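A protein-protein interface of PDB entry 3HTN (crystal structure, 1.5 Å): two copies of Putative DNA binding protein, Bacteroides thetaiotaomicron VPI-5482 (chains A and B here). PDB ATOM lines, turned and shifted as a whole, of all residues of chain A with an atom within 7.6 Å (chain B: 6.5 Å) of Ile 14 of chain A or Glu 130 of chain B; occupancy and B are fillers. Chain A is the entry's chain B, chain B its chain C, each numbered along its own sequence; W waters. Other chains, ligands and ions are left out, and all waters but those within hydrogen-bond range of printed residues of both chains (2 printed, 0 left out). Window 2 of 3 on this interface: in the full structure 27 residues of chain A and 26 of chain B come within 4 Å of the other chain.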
ATOM      1  N   TYR A  11     -13.158 -36.070  18.989  1.00  0.00           N
ATOM      2  CA  TYR A  11     -12.465 -35.066  18.197  1.00  0.00           C
ATOM      3  C   TYR A  11     -13.342 -33.886  17.833  1.00  0.00           C
ATOM      4  O   TYR A  11     -14.585 -33.916  17.939  1.00  0.00           O
ATOM      5  CB  TYR A  11     -11.875 -35.692  16.928  1.00  0.00           C
ATOM      6  CG  TYR A  11     -12.919 -36.132  15.937  1.00  0.00           C
ATOM      7  CD1 TYR A  11     -13.510 -37.376  16.046  1.00  0.00           C
ATOM      8  CD2 TYR A  11     -13.300 -35.299  14.880  1.00  0.00           C
ATOM      9  CE1 TYR A  11     -14.477 -37.782  15.151  1.00  0.00           C
ATOM     10  CE2 TYR A  11     -14.282 -35.690  13.979  1.00  0.00           C
ATOM     11  CZ  TYR A  11     -14.855 -36.929  14.126  1.00  0.00           C
ATOM     12  OH  TYR A  11     -15.808 -37.334  13.221  1.00  0.00           O
ATOM     13  N   LYS A  12     -12.654 -32.843  17.393  1.00  0.00           N
ATOM     14  CA  LYS A  12     -13.269 -31.631  16.926  1.00  0.00           C
ATOM     15  C   LYS A  12     -12.491 -31.197  15.697  1.00  0.00           C
ATOM     16  O   LYS A  12     -11.272 -31.058  15.739  1.00  0.00           O
ATOM     17  CB  LYS A  12     -13.209 -30.556  17.984  1.00  0.00           C
ATOM     18  CG  LYS A  12     -13.835 -29.244  17.502  1.00  0.00           C
ATOM     19  CD  LYS A  12     -13.773 -28.183  18.551  1.00  0.00           C
ATOM     20  CE  LYS A  12     -14.376 -26.905  18.051  1.00  0.00           C
ATOM     21  NZ  LYS A  12     -15.837 -27.066  17.836  1.00  0.00           N
ATOM     22  N   LYS A  13     -13.209 -30.999  14.605  1.00  0.00           N
ATOM     23  CA  LYS A  13     -12.623 -30.542  13.354  1.00  0.00           C
ATOM     24  C   LYS A  13     -12.572 -29.023  13.347  1.00  0.00           C
ATOM     25  O   LYS A  13     -13.602 -28.361  13.591  1.00  0.00           O
ATOM     26  CB  LYS A  13     -13.463 -31.031  12.178  1.00  0.00           C
ATOM     27  CG  LYS A  13     -12.828 -30.777  10.802  1.00  0.00           C
ATOM     28  CD  LYS A  13     -13.792 -31.122   9.693  1.00  0.00           C
ATOM     29  CE  LYS A  13     -13.180 -30.918   8.299  1.00  0.00           C
ATOM     30  NZ  LYS A  13     -13.032 -29.468   7.976  1.00  0.00           N
ATOM     31  N   ILE A  14     -11.398 -28.466  13.082  1.00  0.00           N
ATOM     32  CA  ILE A  14     -11.238 -27.031  12.917  1.00  0.00           C
ATOM     33  C   ILE A  14     -10.475 -26.805  11.623  1.00  0.00           C
ATOM     34  O   ILE A  14      -9.255 -26.891  11.586  1.00  0.00           O
ATOM     35  CB  ILE A  14     -10.523 -26.374  14.086  1.00  0.00           C
ATOM     36  CG1 ILE A  14     -11.261 -26.673  15.393  1.00  0.00           C
ATOM     37  CG2 ILE A  14     -10.449 -24.846  13.838  1.00  0.00           C
ATOM     38  CD1 ILE A  14     -10.579 -26.108  16.598  1.00  0.00           C
ATOM     39  N   GLY A  15     -11.211 -26.514  10.559  1.00  0.00           N
ATOM     40  CA  GLY A  15     -10.610 -26.301   9.264  1.00  0.00           C
ATOM     41  C   GLY A  15      -9.863 -27.543   8.833  1.00  0.00           C
ATOM     42  O   GLY A  15     -10.443 -28.625   8.817  1.00  0.00           O
ATOM     43  N   ASN A  16      -8.577 -27.372   8.528  1.00  0.00           N
ATOM     44  CA  ASN A  16      -7.693 -28.458   8.084  1.00  0.00           C
ATOM     45  C   ASN A  16      -7.087 -29.276   9.220  1.00  0.00           C
ATOM     46  O   ASN A  16      -6.256 -30.129   8.967  1.00  0.00           O
ATOM     47  CB  ASN A  16      -6.544 -27.893   7.213  1.00  0.00           C
ATOM     48  CG  ASN A  16      -5.592 -26.935   7.989  1.00  0.00           C
ATOM     49  OD1 ASN A  16      -5.880 -26.509   9.106  1.00  0.00           O
ATOM     50  ND2 ASN A  16      -4.469 -26.581   7.365  1.00  0.00           N
ATOM     51  N   LYS A  17      -7.498 -29.017  10.453  1.00  0.00           N
ATOM     52  CA  LYS A  17      -6.953 -29.696  11.615  1.00  0.00           C
ATOM     53  C   LYS A  17      -8.044 -30.424  12.363  1.00  0.00           C
ATOM     54  O   LYS A  17      -9.223 -30.096  12.248  1.00  0.00           O
ATOM     55  CB  LYS A  17      -6.313 -28.684  12.555  1.00  0.00           C
ATOM     56  CG  LYS A  17      -5.082 -28.063  11.992  1.00  0.00           C
ATOM     57  CD  LYS A  17      -4.467 -27.091  12.990  1.00  0.00           C
ATOM     58  CE  LYS A  17      -3.401 -26.258  12.324  1.00  0.00           C
ATOM     59  NZ  LYS A  17      -4.025 -25.271  11.392  1.00  0.00           N
ATOM     60  N   TYR A  18      -7.637 -31.435  13.112  1.00  0.00           N
ATOM     61  CA  TYR A  18      -8.500 -32.124  14.050  1.00  0.00           C
ATOM     62  C   TYR A  18      -7.847 -32.077  15.416  1.00  0.00           C
ATOM     63  O   TYR A  18      -6.661 -32.375  15.546  1.00  0.00           O
ATOM     64  CB  TYR A  18      -8.722 -33.575  13.679  1.00  0.00           C
ATOM     65  CG  TYR A  18      -9.456 -33.828  12.375  1.00  0.00           C
ATOM     66  CD1 TYR A  18     -10.842 -33.840  12.329  1.00  0.00           C
ATOM     67  CD2 TYR A  18      -8.749 -34.107  11.205  1.00  0.00           C
ATOM     68  CE1 TYR A  18     -11.500 -34.109  11.157  1.00  0.00           C
ATOM     69  CE2 TYR A  18      -9.403 -34.366  10.028  1.00  0.00           C
ATOM     70  CZ  TYR A  18     -10.766 -34.379  10.009  1.00  0.00           C
ATOM     71  OH  TYR A  18     -11.406 -34.654   8.804  1.00  0.00           O
ATOM     72  N   ILE A  19      -8.616 -31.707  16.423  1.00  0.00           N
ATOM     73  CA  ILE A  19      -8.157 -31.770  17.786  1.00  0.00           C
ATOM     74  C   ILE A  19      -8.687 -33.121  18.281  1.00  0.00           C
ATOM     75  O   ILE A  19      -9.904 -33.347  18.279  1.00  0.00           O
ATOM     76  CB  ILE A  19      -8.695 -30.596  18.625  1.00  0.00           C
ATOM     77  CG1 ILE A  19      -8.426 -29.240  17.940  1.00  0.00           C
ATOM     78  CG2 ILE A  19      -8.102 -30.638  19.993  1.00  0.00           C
ATOM     79  CD1 ILE A  19      -7.023 -29.025  17.411  1.00  0.00           C
ATOM     80  N   VAL A 125      -4.016 -33.101  14.795  1.00  0.00           N
ATOM     81  CA  VAL A 125      -3.747 -33.821  13.566  1.00  0.00           C
ATOM     82  C   VAL A 125      -4.060 -32.865  12.429  1.00  0.00           C
ATOM     83  O   VAL A 125      -5.225 -32.456  12.260  1.00  0.00           O
ATOM     84  CB  VAL A 125      -4.607 -35.070  13.451  1.00  0.00           C
ATOM     85  CG1 VAL A 125      -4.389 -35.757  12.088  1.00  0.00           C
ATOM     86  CG2 VAL A 125      -4.340 -36.007  14.620  1.00  0.00           C
ATOM     87  N   LEU B  42      -9.473 -17.878  21.916  1.00  0.00           N
ATOM     88  CA  LEU B  42     -10.395 -18.896  22.403  1.00  0.00           C
ATOM     89  C   LEU B  42      -9.733 -20.275  22.574  1.00  0.00           C
ATOM     90  O   LEU B  42      -9.933 -20.996  23.557  1.00  0.00           O
ATOM     91  CB  LEU B  42     -11.566 -18.983  21.404  1.00  0.00           C
ATOM     92  CG  LEU B  42     -12.470 -17.744  21.292  1.00  0.00           C
ATOM     93  CD1 LEU B  42     -13.352 -17.782  20.041  1.00  0.00           C
ATOM     94  CD2 LEU B  42     -13.273 -17.647  22.561  1.00  0.00           C
ATOM     95  N   SER B  43      -8.984 -20.657  21.557  1.00  0.00           N
ATOM     96  CA  SER B  43      -8.316 -21.940  21.497  1.00  0.00           C
ATOM     97  C   SER B  43      -7.224 -21.834  20.478  1.00  0.00           C
ATOM     98  O   SER B  43      -7.209 -20.932  19.663  1.00  0.00           O
ATOM     99  CB  SER B  43      -9.267 -23.094  21.134  1.00  0.00           C
ATOM    100  OG  SER B  43      -9.710 -23.000  19.784  1.00  0.00           O
ATOM    101  N   GLY B  44      -6.288 -22.770  20.549  1.00  0.00           N
ATOM    102  CA  GLY B  44      -5.128 -22.729  19.689  1.00  0.00           C
ATOM    103  C   GLY B  44      -4.012 -23.572  20.237  1.00  0.00           C
ATOM    104  O   GLY B  44      -4.219 -24.400  21.131  1.00  0.00           O
ATOM    105  N   ILE B  85      -4.373 -24.263  23.975  1.00  0.00           N
ATOM    106  CA  ILE B  85      -5.211 -23.218  24.535  1.00  0.00           C
ATOM    107  C   ILE B  85      -6.650 -23.674  24.396  1.00  0.00           C
ATOM    108  O   ILE B  85      -7.043 -24.196  23.342  1.00  0.00           O
ATOM    109  CB  ILE B  85      -5.022 -21.898  23.776  1.00  0.00           C
ATOM    110  CG1 ILE B  85      -3.555 -21.484  23.674  1.00  0.00           C
ATOM    111  CG2 ILE B  85      -5.859 -20.752  24.413  1.00  0.00           C
ATOM    112  CD1 ILE B  85      -3.257 -20.482  22.606  1.00  0.00           C
ATOM    113  N   ASP B 127      -3.975 -19.207  16.597  1.00  0.00           N
ATOM    114  CA  ASP B 127      -5.328 -18.929  17.048  1.00  0.00           C
ATOM    115  C   ASP B 127      -6.310 -19.683  16.154  1.00  0.00           C
ATOM    116  O   ASP B 127      -6.411 -19.374  14.975  1.00  0.00           O
ATOM    117  CB  ASP B 127      -5.541 -17.419  16.938  1.00  0.00           C
ATOM    118  CG  ASP B 127      -6.900 -16.958  17.390  1.00  0.00           C
ATOM    119  OD1 ASP B 127      -7.735 -17.764  17.859  1.00  0.00           O
ATOM    120  OD2 ASP B 127      -7.138 -15.724  17.258  1.00  0.00           O
ATOM    121  N   TYR B 128      -7.048 -20.615  16.738  1.00  0.00           N
ATOM    122  CA  TYR B 128      -8.059 -21.375  15.998  1.00  0.00           C
ATOM    123  C   TYR B 128      -9.379 -20.648  15.825  1.00  0.00           C
ATOM    124  O   TYR B 128     -10.200 -21.112  15.049  1.00  0.00           O
ATOM    125  CB  TYR B 128      -8.376 -22.705  16.681  1.00  0.00           C
ATOM    126  CG  TYR B 128      -7.248 -23.684  16.873  1.00  0.00           C
ATOM    127  CD1 TYR B 128      -6.110 -23.685  16.075  1.00  0.00           C
ATOM    128  CD2 TYR B 128      -7.355 -24.665  17.830  1.00  0.00           C
ATOM    129  CE1 TYR B 128      -5.102 -24.608  16.278  1.00  0.00           C
ATOM    130  CE2 TYR B 128      -6.383 -25.583  18.026  1.00  0.00           C
ATOM    131  CZ  TYR B 128      -5.254 -25.552  17.266  1.00  0.00           C
ATOM    132  OH  TYR B 128      -4.275 -26.505  17.493  1.00  0.00           O
ATOM    133  N   SER B 129      -9.618 -19.558  16.556  1.00  0.00           N
ATOM    134  CA  SER B 129     -10.861 -18.793  16.426  1.00  0.00           C
ATOM    135  C   SER B 129     -12.115 -19.618  16.661  1.00  0.00           C
ATOM    136  O   SER B 129     -13.147 -19.353  16.042  1.00  0.00           O
ATOM    137  CB  SER B 129     -10.925 -18.139  15.041  1.00  0.00           C
ATOM    138  OG  SER B 129      -9.899 -17.192  14.885  1.00  0.00           O
ATOM    139  N   GLU B 130     -11.970 -20.653  17.456  1.00  0.00           N
ATOM    140  CA  GLU B 130     -12.976 -21.644  17.681  1.00  0.00           C
ATOM    141  C   GLU B 130     -12.888 -21.948  19.135  1.00  0.00           C
ATOM    142  O   GLU B 130     -11.834 -22.195  19.693  1.00  0.00           O
ATOM    143  CB  GLU B 130     -12.715 -22.927  16.899  1.00  0.00           C
ATOM    144  CG  GLU B 130     -13.023 -22.850  15.433  1.00  0.00           C
ATOM    145  CD  GLU B 130     -14.500 -22.692  15.124  1.00  0.00           C
ATOM    146  OE1 GLU B 130     -15.347 -22.937  16.013  1.00  0.00           O
ATOM    147  OE2 GLU B 130     -14.802 -22.327  13.972  1.00  0.00           O
ATOM    148  N   ARG B 131     -14.492 -21.697  20.165  1.00  0.00           N
ATOM    149  CA  ARG B 131     -14.596 -22.152  21.540  1.00  0.00           C
ATOM    150  C   ARG B 131     -14.200 -23.625  21.629  1.00  0.00           C
ATOM    151  O   ARG B 131     -14.729 -24.439  20.871  1.00  0.00           O
ATOM    152  CB  ARG B 131     -16.047 -21.956  22.008  1.00  0.00           C
ATOM    153  CG  ARG B 131     -16.350 -22.257  23.471  1.00  0.00           C
ATOM    154  CD  ARG B 131     -15.655 -21.263  24.403  1.00  0.00           C
ATOM    155  NE  ARG B 131     -16.068 -19.863  24.253  1.00  0.00           N
ATOM    156  CZ  ARG B 131     -15.432 -18.818  24.797  1.00  0.00           C
ATOM    157  NH1 ARG B 131     -15.911 -17.577  24.612  1.00  0.00           N
ATOM    158  NH2 ARG B 131     -14.317 -18.994  25.532  1.00  0.00           N
ATOM    159  N   ILE B 132     -13.241 -23.958  22.504  1.00  0.00           N
ATOM    160  CA  ILE B 132     -12.970 -25.362  22.903  1.00  0.00           C
ATOM    161  C   ILE B 132     -12.957 -25.359  24.417  1.00  0.00           C
ATOM    162  O   ILE B 132     -12.151 -24.632  25.027  1.00  0.00           O
ATOM    163  CB  ILE B 132     -11.633 -25.957  22.432  1.00  0.00           C
ATOM    164  CG1 ILE B 132     -11.552 -25.988  20.908  1.00  0.00           C
ATOM    165  CG2 ILE B 132     -11.459 -27.377  22.989  1.00  0.00           C
ATOM    166  CD1 ILE B 132     -10.253 -26.536  20.398  1.00  0.00           C
HETATM  167  O   HOH W   1     -16.294 -24.163  18.535  1.00  0.00           O
HETATM  168  O   HOH W   2     -15.867 -27.166  21.075  1.00  0.00           O
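Of the 10 printed residues of chain B, 4 touch a printed residue of chain A.
Of the 10 printed residues of chain A, 3 touch a printed residue of chain B.
No position is printed for both chains.
Of the 6 pairs that touch across the chains among the printed residues, none has its exchanged pair printed and touching as well.
The backbone NH (N) of Ile 19 of chain A lies within hydrogen-bond range of the backbone carbonyl oxygen (O) of Lys 12 of chain A (2.8 Å).
O of Ser 43 of chain B is in hydrogen-bond range of N of Tyr 128 of chain B.
Printed residues of chain B within 4 Å of Ile 14 of chain A: Tyr 128, Glu 130 and Ile 132.
Of the printed residues of chain B, Lys 12 of chain A touches Arg 131 and Ile 132.
Printed residues of chain B within 4 Å of Ile 19 of chain A: Tyr 128.
Lys 13 of chain A touches none of the printed residues of chain B.
Leu 42 of chain B touches none of the printed residues of chain A.
Among the printed residues, pairs that only touch across the chains: Lys 12 of chain A with Arg 131 of chain B (3.8 Å), Lys 12 of chain A with Ile 132 of chain B (3.9 Å), Ile 14 of chain A with Tyr 128 of chain B (3.7 Å), Ile 14 of chain A with Glu 130 of chain B (3.6 Å), Ile 14 of chain A with Ile 132 of chain B (3.8 Å) and Ile 19 of chain A with Tyr 128 of chain B (3.6 Å).
Water W1 lies within hydrogen-bond range of the backbone carbonyl oxygen (O) of Arg 131 of chain B, the side-chain carboxylate (OE1) of Glu 130 of chain B and the side-chain amino group (NZ) of Lys 12 of chain A.
Water W2 lies within hydrogen-bond range of the backbone carbonyl oxygen (O) of Arg 131 of chain B (3.0 Å) and the side-chain amino group (NZ) of Lys 12 of chain A (3.2 Å).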
